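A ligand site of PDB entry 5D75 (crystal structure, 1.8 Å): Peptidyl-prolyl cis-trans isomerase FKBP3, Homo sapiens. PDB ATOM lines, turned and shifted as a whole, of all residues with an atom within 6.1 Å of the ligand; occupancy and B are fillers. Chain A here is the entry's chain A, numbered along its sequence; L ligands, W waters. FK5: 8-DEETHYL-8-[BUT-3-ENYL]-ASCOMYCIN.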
ATOM      1  N   TYR A  27     -17.434 -24.101  -6.198  1.00  0.00           N
ATOM      2  CA  TYR A  27     -17.143 -24.047  -4.761  1.00  0.00           C
ATOM      3  C   TYR A  27     -17.534 -22.747  -4.095  1.00  0.00           C
ATOM      4  O   TYR A  27     -17.608 -21.717  -4.770  1.00  0.00           O
ATOM      5  CB  TYR A  27     -15.663 -24.328  -4.503  1.00  0.00           C
ATOM      6  CG  TYR A  27     -14.757 -23.222  -4.947  1.00  0.00           C
ATOM      7  CD1 TYR A  27     -14.242 -23.185  -6.256  1.00  0.00           C
ATOM      8  CD2 TYR A  27     -14.404 -22.186  -4.064  1.00  0.00           C
ATOM      9  CE1 TYR A  27     -13.427 -22.156  -6.678  1.00  0.00           C
ATOM     10  CE2 TYR A  27     -13.593 -21.139  -4.480  1.00  0.00           C
ATOM     11  CZ  TYR A  27     -13.114 -21.133  -5.780  1.00  0.00           C
ATOM     12  OH  TYR A  27     -12.288 -20.131  -6.177  1.00  0.00           O
ATOM     13  N   GLY A  29     -16.068 -20.988  -0.367  1.00  0.00           N
ATOM     14  CA  GLY A  29     -15.220 -21.077   0.819  1.00  0.00           C
ATOM     15  C   GLY A  29     -15.658 -20.120   1.924  1.00  0.00           C
ATOM     16  O   GLY A  29     -15.879 -18.899   1.670  1.00  0.00           O
ATOM     17  N   PHE A  37     -15.032 -16.085   1.931  1.00  0.00           N
ATOM     18  CA  PHE A  37     -13.817 -15.498   1.379  1.00  0.00           C
ATOM     19  C   PHE A  37     -13.722 -15.663  -0.125  1.00  0.00           C
ATOM     20  O   PHE A  37     -12.979 -14.933  -0.786  1.00  0.00           O
ATOM     21  CB  PHE A  37     -12.538 -16.009   2.087  1.00  0.00           C
ATOM     22  CG  PHE A  37     -12.354 -17.503   2.038  1.00  0.00           C
ATOM     23  CD1 PHE A  37     -11.824 -18.132   0.890  1.00  0.00           C
ATOM     24  CD2 PHE A  37     -12.712 -18.299   3.147  1.00  0.00           C
ATOM     25  CE1 PHE A  37     -11.649 -19.527   0.860  1.00  0.00           C
ATOM     26  CE2 PHE A  37     -12.529 -19.682   3.120  1.00  0.00           C
ATOM     27  CZ  PHE A  37     -11.994 -20.291   1.979  1.00  0.00           C
ATOM     28  N   ASP A  38     -14.447 -16.624  -0.680  1.00  0.00           N
ATOM     29  CA  ASP A  38     -14.408 -16.860  -2.126  1.00  0.00           C
ATOM     30  C   ASP A  38     -15.528 -17.743  -2.572  1.00  0.00           C
ATOM     31  O   ASP A  38     -16.038 -18.590  -1.814  1.00  0.00           O
ATOM     32  CB  ASP A  38     -13.087 -17.504  -2.551  1.00  0.00           C
ATOM     33  CG  ASP A  38     -12.814 -17.399  -4.056  1.00  0.00           C
ATOM     34  OD1 ASP A  38     -13.477 -16.596  -4.779  1.00  0.00           O
ATOM     35  OD2 ASP A  38     -11.894 -18.113  -4.532  1.00  0.00           O
ATOM     36  N   THR A  39     -15.906 -17.548  -3.828  1.00  0.00           N
ATOM     37  CA  THR A  39     -16.760 -18.468  -4.548  1.00  0.00           C
ATOM     38  C   THR A  39     -16.485 -18.324  -6.042  1.00  0.00           C
ATOM     39  O   THR A  39     -16.112 -17.244  -6.523  1.00  0.00           O
ATOM     40  CB  THR A  39     -18.257 -18.283  -4.208  1.00  0.00           C
ATOM     41  OG1 THR A  39     -19.011 -19.262  -4.907  1.00  0.00           O
ATOM     42  CG2 THR A  39     -18.773 -16.850  -4.610  1.00  0.00           C
ATOM     43  N   LEU A  54     -14.098 -24.449 -11.850  1.00  0.00           N
ATOM     44  CA  LEU A  54     -12.656 -24.498 -11.695  1.00  0.00           C
ATOM     45  C   LEU A  54     -12.154 -25.856 -12.181  1.00  0.00           C
ATOM     46  O   LEU A  54     -12.715 -26.908 -11.790  1.00  0.00           O
ATOM     47  CB  LEU A  54     -12.258 -24.261 -10.227  1.00  0.00           C
ATOM     48  CG  LEU A  54     -10.791 -24.539  -9.876  1.00  0.00           C
ATOM     49  CD1 LEU A  54      -9.868 -23.423 -10.379  1.00  0.00           C
ATOM     50  CD2 LEU A  54     -10.654 -24.756  -8.383  1.00  0.00           C
ATOM     51  N   PHE A  56      -8.709 -28.368 -12.516  1.00  0.00           N
ATOM     52  CA  PHE A  56      -7.322 -28.634 -12.114  1.00  0.00           C
ATOM     53  C   PHE A  56      -7.039 -30.126 -12.134  1.00  0.00           C
ATOM     54  O   PHE A  56      -7.963 -30.955 -12.017  1.00  0.00           O
ATOM     55  CB  PHE A  56      -7.006 -28.043 -10.727  1.00  0.00           C
ATOM     56  CG  PHE A  56      -7.800 -28.638  -9.602  1.00  0.00           C
ATOM     57  CD1 PHE A  56      -9.065 -28.125  -9.274  1.00  0.00           C
ATOM     58  CD2 PHE A  56      -7.287 -29.712  -8.855  1.00  0.00           C
ATOM     59  CE1 PHE A  56      -9.804 -28.686  -8.229  1.00  0.00           C
ATOM     60  CE2 PHE A  56      -8.016 -30.271  -7.809  1.00  0.00           C
ATOM     61  CZ  PHE A  56      -9.273 -29.742  -7.496  1.00  0.00           C
ATOM     62  N   GLY A  61      -0.651 -31.802  -6.018  1.00  0.00           N
ATOM     63  CA  GLY A  61      -0.212 -30.587  -5.337  1.00  0.00           C
ATOM     64  C   GLY A  61      -0.620 -29.261  -5.960  1.00  0.00           C
ATOM     65  O   GLY A  61      -0.091 -28.230  -5.577  1.00  0.00           O
ATOM     66  N   LYS A  62      -1.585 -29.280  -6.884  1.00  0.00           N
ATOM     67  CA  LYS A  62      -2.054 -28.052  -7.541  1.00  0.00           C
ATOM     68  C   LYS A  62      -3.058 -27.252  -6.680  1.00  0.00           C
ATOM     69  O   LYS A  62      -3.312 -26.078  -6.940  1.00  0.00           O
ATOM     70  CB  LYS A  62      -2.658 -28.344  -8.925  1.00  0.00           C
ATOM     71  CG  LYS A  62      -1.627 -28.828  -9.951  1.00  0.00           C
ATOM     72  CD  LYS A  62      -0.706 -27.718 -10.435  1.00  0.00           C
ATOM     73  CE  LYS A  62       0.163 -28.164 -11.608  1.00  0.00           C
ATOM     74  NZ  LYS A  62       1.223 -29.178 -11.315  1.00  0.00           N
ATOM     75  N   VAL A  63      -3.612 -27.912  -5.672  1.00  0.00           N
ATOM     76  CA  VAL A  63      -4.574 -27.278  -4.753  1.00  0.00           C
ATOM     77  C   VAL A  63      -4.142 -27.567  -3.312  1.00  0.00           C
ATOM     78  O   VAL A  63      -3.267 -28.395  -3.103  1.00  0.00           O
ATOM     79  CB  VAL A  63      -6.018 -27.750  -4.978  1.00  0.00           C
ATOM     80  CG1 VAL A  63      -6.569 -27.209  -6.312  1.00  0.00           C
ATOM     81  CG2 VAL A  63      -6.134 -29.273  -4.879  1.00  0.00           C
ATOM     82  N   ILE A  64      -4.744 -26.860  -2.345  1.00  0.00           N
ATOM     83  CA  ILE A  64      -4.475 -27.133  -0.931  1.00  0.00           C
ATOM     84  C   ILE A  64      -4.750 -28.603  -0.610  1.00  0.00           C
ATOM     85  O   ILE A  64      -5.602 -29.252  -1.240  1.00  0.00           O
ATOM     86  CB  ILE A  64      -5.223 -26.183   0.044  1.00  0.00           C
ATOM     87  CG1 ILE A  64      -6.743 -26.198  -0.209  1.00  0.00           C
ATOM     88  CG2 ILE A  64      -4.656 -24.772  -0.075  1.00  0.00           C
ATOM     89  CD1 ILE A  64      -7.581 -25.623   0.942  1.00  0.00           C
ATOM     90  N   TRP A  67      -8.295 -30.270  -0.286  1.00  0.00           N
ATOM     91  CA  TRP A  67      -8.960 -30.516  -1.578  1.00  0.00           C
ATOM     92  C   TRP A  67      -8.378 -31.716  -2.346  1.00  0.00           C
ATOM     93  O   TRP A  67      -9.145 -32.533  -2.841  1.00  0.00           O
ATOM     94  CB  TRP A  67      -8.827 -29.290  -2.462  1.00  0.00           C
ATOM     95  CG  TRP A  67      -9.892 -28.290  -2.290  1.00  0.00           C
ATOM     96  CD1 TRP A  67     -10.189 -27.574  -1.162  1.00  0.00           C
ATOM     97  CD2 TRP A  67     -10.832 -27.869  -3.291  1.00  0.00           C
ATOM     98  NE1 TRP A  67     -11.240 -26.713  -1.395  1.00  0.00           N
ATOM     99  CE2 TRP A  67     -11.663 -26.877  -2.686  1.00  0.00           C
ATOM    100  CE3 TRP A  67     -11.051 -28.232  -4.626  1.00  0.00           C
ATOM    101  CZ2 TRP A  67     -12.700 -26.231  -3.389  1.00  0.00           C
ATOM    102  CZ3 TRP A  67     -12.078 -27.582  -5.337  1.00  0.00           C
ATOM    103  CH2 TRP A  67     -12.889 -26.602  -4.713  1.00  0.00           C
ATOM    104  N   ALA A  89      -4.617 -26.623   4.713  1.00  0.00           N
ATOM    105  CA  ALA A  89      -5.090 -25.441   3.990  1.00  0.00           C
ATOM    106  C   ALA A  89      -3.929 -24.447   3.950  1.00  0.00           C
ATOM    107  O   ALA A  89      -2.898 -24.763   3.349  1.00  0.00           O
ATOM    108  CB  ALA A  89      -6.321 -24.864   4.684  1.00  0.00           C
ATOM    109  N   TYR A  90      -4.060 -23.277   4.597  1.00  0.00           N
ATOM    110  CA  TYR A  90      -2.995 -22.245   4.540  1.00  0.00           C
ATOM    111  C   TYR A  90      -2.115 -22.157   5.801  1.00  0.00           C
ATOM    112  O   TYR A  90      -1.179 -21.340   5.849  1.00  0.00           O
ATOM    113  CB  TYR A  90      -3.583 -20.869   4.137  1.00  0.00           C
ATOM    114  CG  TYR A  90      -4.094 -20.913   2.728  1.00  0.00           C
ATOM    115  CD1 TYR A  90      -3.213 -20.740   1.664  1.00  0.00           C
ATOM    116  CD2 TYR A  90      -5.436 -21.169   2.449  1.00  0.00           C
ATOM    117  CE1 TYR A  90      -3.653 -20.796   0.351  1.00  0.00           C
ATOM    118  CE2 TYR A  90      -5.891 -21.246   1.128  1.00  0.00           C
ATOM    119  CZ  TYR A  90      -4.977 -21.054   0.093  1.00  0.00           C
ATOM    120  OH  TYR A  90      -5.353 -21.118  -1.218  1.00  0.00           O
ATOM    121  N   GLN A  95      -3.615 -16.601   4.258  1.00  0.00           N
ATOM    122  CA  GLN A  95      -3.548 -16.075   2.913  1.00  0.00           C
ATOM    123  C   GLN A  95      -4.056 -14.627   2.997  1.00  0.00           C
ATOM    124  O   GLN A  95      -5.261 -14.404   3.077  1.00  0.00           O
ATOM    125  CB  GLN A  95      -4.382 -16.935   1.951  1.00  0.00           C
ATOM    126  CG  GLN A  95      -3.757 -17.003   0.567  1.00  0.00           C
ATOM    127  CD  GLN A  95      -3.759 -15.667  -0.128  1.00  0.00           C
ATOM    128  OE1 GLN A  95      -4.798 -14.997  -0.197  1.00  0.00           O
ATOM    129  NE2 GLN A  95      -2.602 -15.251  -0.641  1.00  0.00           N
ATOM    130  N   ASP A  97      -4.264 -11.980   0.895  1.00  0.00           N
ATOM    131  CA  ASP A  97      -5.108 -11.416  -0.172  1.00  0.00           C
ATOM    132  C   ASP A  97      -6.570 -11.798  -0.048  1.00  0.00           C
ATOM    133  O   ASP A  97      -7.444 -11.011  -0.374  1.00  0.00           O
ATOM    134  CB  ASP A  97      -4.571 -11.799  -1.551  1.00  0.00           C
ATOM    135  CG  ASP A  97      -3.104 -11.564  -1.676  1.00  0.00           C
ATOM    136  OD1 ASP A  97      -2.306 -12.439  -1.278  1.00  0.00           O
ATOM    137  OD2 ASP A  97      -2.758 -10.468  -2.123  1.00  0.00           O
ATOM    138  N   ALA A  98      -6.828 -13.013   0.433  1.00  0.00           N
ATOM    139  CA  ALA A  98      -8.182 -13.488   0.632  1.00  0.00           C
ATOM    140  C   ALA A  98      -8.664 -13.212   2.056  1.00  0.00           C
ATOM    141  O   ALA A  98      -9.775 -13.606   2.411  1.00  0.00           O
ATOM    142  CB  ALA A  98      -8.241 -14.982   0.325  1.00  0.00           C
ATOM    143  N   ILE A 100      -7.573 -14.612   4.756  1.00  0.00           N
ATOM    144  CA  ILE A 100      -7.608 -15.819   5.570  1.00  0.00           C
ATOM    145  C   ILE A 100      -6.529 -15.683   6.651  1.00  0.00           C
ATOM    146  O   ILE A 100      -5.349 -15.590   6.327  1.00  0.00           O
ATOM    147  CB  ILE A 100      -7.433 -17.092   4.718  1.00  0.00           C
ATOM    148  CG1 ILE A 100      -8.695 -17.264   3.853  1.00  0.00           C
ATOM    149  CG2 ILE A 100      -7.148 -18.306   5.606  1.00  0.00           C
ATOM    150  CD1 ILE A 100      -8.543 -18.278   2.742  1.00  0.00           C
ATOM    151  N   LEU A 106     -10.884 -24.121   7.342  1.00  0.00           N
ATOM    152  CA  LEU A 106     -11.690 -23.615   6.209  1.00  0.00           C
ATOM    153  C   LEU A 106     -12.838 -24.552   5.901  1.00  0.00           C
ATOM    154  O   LEU A 106     -12.668 -25.784   5.928  1.00  0.00           O
ATOM    155  CB  LEU A 106     -10.818 -23.434   4.958  1.00  0.00           C
ATOM    156  CG  LEU A 106      -9.575 -22.552   5.079  1.00  0.00           C
ATOM    157  CD1 LEU A 106      -8.946 -22.407   3.695  1.00  0.00           C
ATOM    158  CD2 LEU A 106      -9.903 -21.188   5.716  1.00  0.00           C
ATOM    159  N   PHE A 108     -15.387 -25.570   2.843  1.00  0.00           N
ATOM    160  CA  PHE A 108     -15.716 -25.413   1.422  1.00  0.00           C
ATOM    161  C   PHE A 108     -16.902 -26.286   1.078  1.00  0.00           C
ATOM    162  O   PHE A 108     -16.941 -27.462   1.472  1.00  0.00           O
ATOM    163  CB  PHE A 108     -14.555 -25.853   0.523  1.00  0.00           C
ATOM    164  CG  PHE A 108     -13.391 -24.914   0.457  1.00  0.00           C
ATOM    165  CD1 PHE A 108     -13.325 -23.936  -0.537  1.00  0.00           C
ATOM    166  CD2 PHE A 108     -12.288 -25.063   1.330  1.00  0.00           C
ATOM    167  CE1 PHE A 108     -12.232 -23.084  -0.645  1.00  0.00           C
ATOM    168  CE2 PHE A 108     -11.194 -24.222   1.220  1.00  0.00           C
ATOM    169  CZ  PHE A 108     -11.150 -23.228   0.229  1.00  0.00           C
HETATM  170  C1  FK5 L   1      -6.825 -23.884  -3.914  1.00  0.00           C
HETATM  171  C2  FK5 L   1      -8.105 -23.701  -3.172  1.00  0.00           C
HETATM  172  C3  FK5 L   1      -9.016 -24.903  -3.457  1.00  0.00           C
HETATM  173  C4  FK5 L   1      -9.647 -24.811  -4.835  1.00  0.00           C
HETATM  174  C5  FK5 L   1     -10.435 -23.494  -4.946  1.00  0.00           C
HETATM  175  C6  FK5 L   1      -9.531 -22.265  -4.727  1.00  0.00           C
HETATM  176  C8  FK5 L   1      -8.775 -21.508  -2.423  1.00  0.00           C
HETATM  177  C9  FK5 L   1      -9.571 -20.267  -2.536  1.00  0.00           C
HETATM  178  C10 FK5 L   1      -8.869 -18.948  -2.870  1.00  0.00           C
HETATM  179  C11 FK5 L   1      -7.699 -18.597  -1.917  1.00  0.00           C
HETATM  180  C12 FK5 L   1      -7.006 -17.290  -2.329  1.00  0.00           C
HETATM  181  C13 FK5 L   1      -6.554 -17.310  -3.784  1.00  0.00           C
HETATM  182  C14 FK5 L   1      -7.656 -17.837  -4.700  1.00  0.00           C
HETATM  183  C15 FK5 L   1      -7.195 -18.038  -6.145  1.00  0.00           C
HETATM  184  C16 FK5 L   1      -8.384 -18.647  -6.904  1.00  0.00           C
HETATM  185  C17 FK5 L   1      -8.076 -19.182  -8.291  1.00  0.00           C
HETATM  186  C18 FK5 L   1      -7.537 -18.108  -9.274  1.00  0.00           C
HETATM  187  C19 FK5 L   1      -6.509 -18.824 -10.117  1.00  0.00           C
HETATM  188  C20 FK5 L   1      -5.225 -18.862  -9.699  1.00  0.00           C
HETATM  189  C21 FK5 L   1      -4.139 -19.624 -10.448  1.00  0.00           C
HETATM  190  C22 FK5 L   1      -3.737 -20.797  -9.581  1.00  0.00           C
HETATM  191  C23 FK5 L   1      -4.658 -21.997  -9.458  1.00  0.00           C
HETATM  192  C24 FK5 L   1      -4.476 -22.759  -8.143  1.00  0.00           C
HETATM  193  C25 FK5 L   1      -5.667 -22.579  -7.207  1.00  0.00           C
HETATM  194  C26 FK5 L   1      -5.409 -23.189  -5.810  1.00  0.00           C
HETATM  195  C27 FK5 L   1      -4.235 -22.601  -5.059  1.00  0.00           C
HETATM  196  C28 FK5 L   1      -3.200 -23.423  -4.753  1.00  0.00           C
HETATM  197  C29 FK5 L   1      -1.952 -23.022  -4.000  1.00  0.00           C
HETATM  198  C30 FK5 L   1      -1.949 -23.645  -2.594  1.00  0.00           C
HETATM  199  C31 FK5 L   1      -0.632 -23.360  -1.828  1.00  0.00           C
HETATM  200  C32 FK5 L   1       0.566 -23.834  -2.651  1.00  0.00           C
HETATM  201  C33 FK5 L   1       0.614 -23.258  -4.077  1.00  0.00           C
HETATM  202  C34 FK5 L   1      -0.721 -23.443  -4.836  1.00  0.00           C
HETATM  203  C35 FK5 L   1      -8.103 -18.505  -0.457  1.00  0.00           C
HETATM  204  C36 FK5 L   1      -9.311 -19.958  -8.788  1.00  0.00           C
HETATM  205  C37 FK5 L   1      -6.966 -19.506 -11.396  1.00  0.00           C
HETATM  206  C38 FK5 L   1      -2.952 -18.742 -10.863  1.00  0.00           C
HETATM  207  C39 FK5 L   1      -3.302 -17.870 -12.055  1.00  0.00           C
HETATM  208  C40 FK5 L   1      -3.233 -18.384 -13.276  1.00  0.00           C
HETATM  209  C41 FK5 L   1      -6.970 -23.116  -7.817  1.00  0.00           C
HETATM  210  C42 FK5 L   1      -4.296 -21.141  -4.646  1.00  0.00           C
HETATM  211  C43 FK5 L   1      -4.907 -15.530  -3.809  1.00  0.00           C
HETATM  212  C44 FK5 L   1      -4.765 -18.027  -6.453  1.00  0.00           C
HETATM  213  C45 FK5 L   1      -0.831 -23.194   0.588  1.00  0.00           C
HETATM  214  N7  FK5 L   1      -8.810 -22.413  -3.422  1.00  0.00           N
HETATM  215  O1  FK5 L   1      -6.589 -23.013  -5.042  1.00  0.00           O
HETATM  216  O2  FK5 L   1      -5.994 -24.740  -3.561  1.00  0.00           O
HETATM  217  O3  FK5 L   1      -8.108 -21.678  -1.388  1.00  0.00           O
HETATM  218  O4  FK5 L   1     -10.786 -20.299  -2.343  1.00  0.00           O
HETATM  219  O5  FK5 L   1      -8.329 -19.039  -4.194  1.00  0.00           O
HETATM  220  O6  FK5 L   1      -9.864 -17.928  -2.791  1.00  0.00           O
HETATM  221  O7  FK5 L   1      -6.194 -15.982  -4.256  1.00  0.00           O
HETATM  222  O8  FK5 L   1      -5.972 -18.791  -6.286  1.00  0.00           O
HETATM  223  O9  FK5 L   1      -2.684 -20.822  -8.967  1.00  0.00           O
HETATM  224  O10 FK5 L   1      -4.275 -24.152  -8.463  1.00  0.00           O
HETATM  225  O11 FK5 L   1      -0.604 -24.027  -0.548  1.00  0.00           O
HETATM  226  O12 FK5 L   1       1.755 -23.459  -1.961  1.00  0.00           O
HETATM  227  O   HOH W   1      -4.633 -25.224 -11.050  1.00  0.00           O
HETATM  228  O   HOH W   2       2.234 -21.023  -0.846  1.00  0.00           O
HETATM  229  O   HOH W   3       0.309 -21.495   3.334  1.00  0.00           O
HETATM  230  O   HOH W   4      -0.711 -26.617  -0.260  1.00  0.00           O
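The backbone carbonyl oxygen of Lys 62 is in hydrogen-bond range of an oxygen (O10) of the ligand (2.6 Å).
O6 of the ligand sits at hydrogen-bond distance from OD2 of Asp 38 (2.7 Å).
O2 of the ligand sits at hydrogen-bond distance from N of Ile 64 (2.7 Å).
O3 of the ligand sits at hydrogen-bond distance from OH of Tyr 90 (2.8 Å).
The side-chain carboxylate of Asp 38 is in hydrogen-bond range of the side-chain hydroxyl of Tyr 27, 2.6 Å away.
O of Asp 38 is in hydrogen-bond range of N of Gly 29.
N of Ile 100 sits at hydrogen-bond distance from O of Gln 95 (2.9 Å).
The backbone carbonyl oxygen (O) of Gly 29 lies within hydrogen-bond range of the backbone NH (N) of Phe 37 (3.0 Å).
The backbone NH (N) of Ala 98 sits at hydrogen-bond distance from the side-chain amide oxygen (OE1) of Gln 95, 2.9 Å away.
The side-chain hydroxyl (OG1) of Thr 39 lies within hydrogen-bond range of the backbone carbonyl oxygen (O) of Tyr 27 (2.8 Å).
OD1 of Asp 97 lies within hydrogen-bond range of NE2 of Gln 95, at 2.9 Å.
Residues that only touch the ligand: Val 63, Ile 100, Trp 67, Phe 37, Phe 108, Ala 98, Tyr 27, Gln 95, Leu 54 and Ala 89.
Hydrophobic or aromatic side chains that line the ligand: Tyr 27, Phe 37, Leu 54, Val 63, Ile 64, Trp 67, Tyr 90, Ala 98, Ile 100 and Phe 108.
Of the 20 residues printed, 14 come within 4 Å of the ligand.
The nearest printed residue that does not touch the ligand is Asp 97 (4.4 Å).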
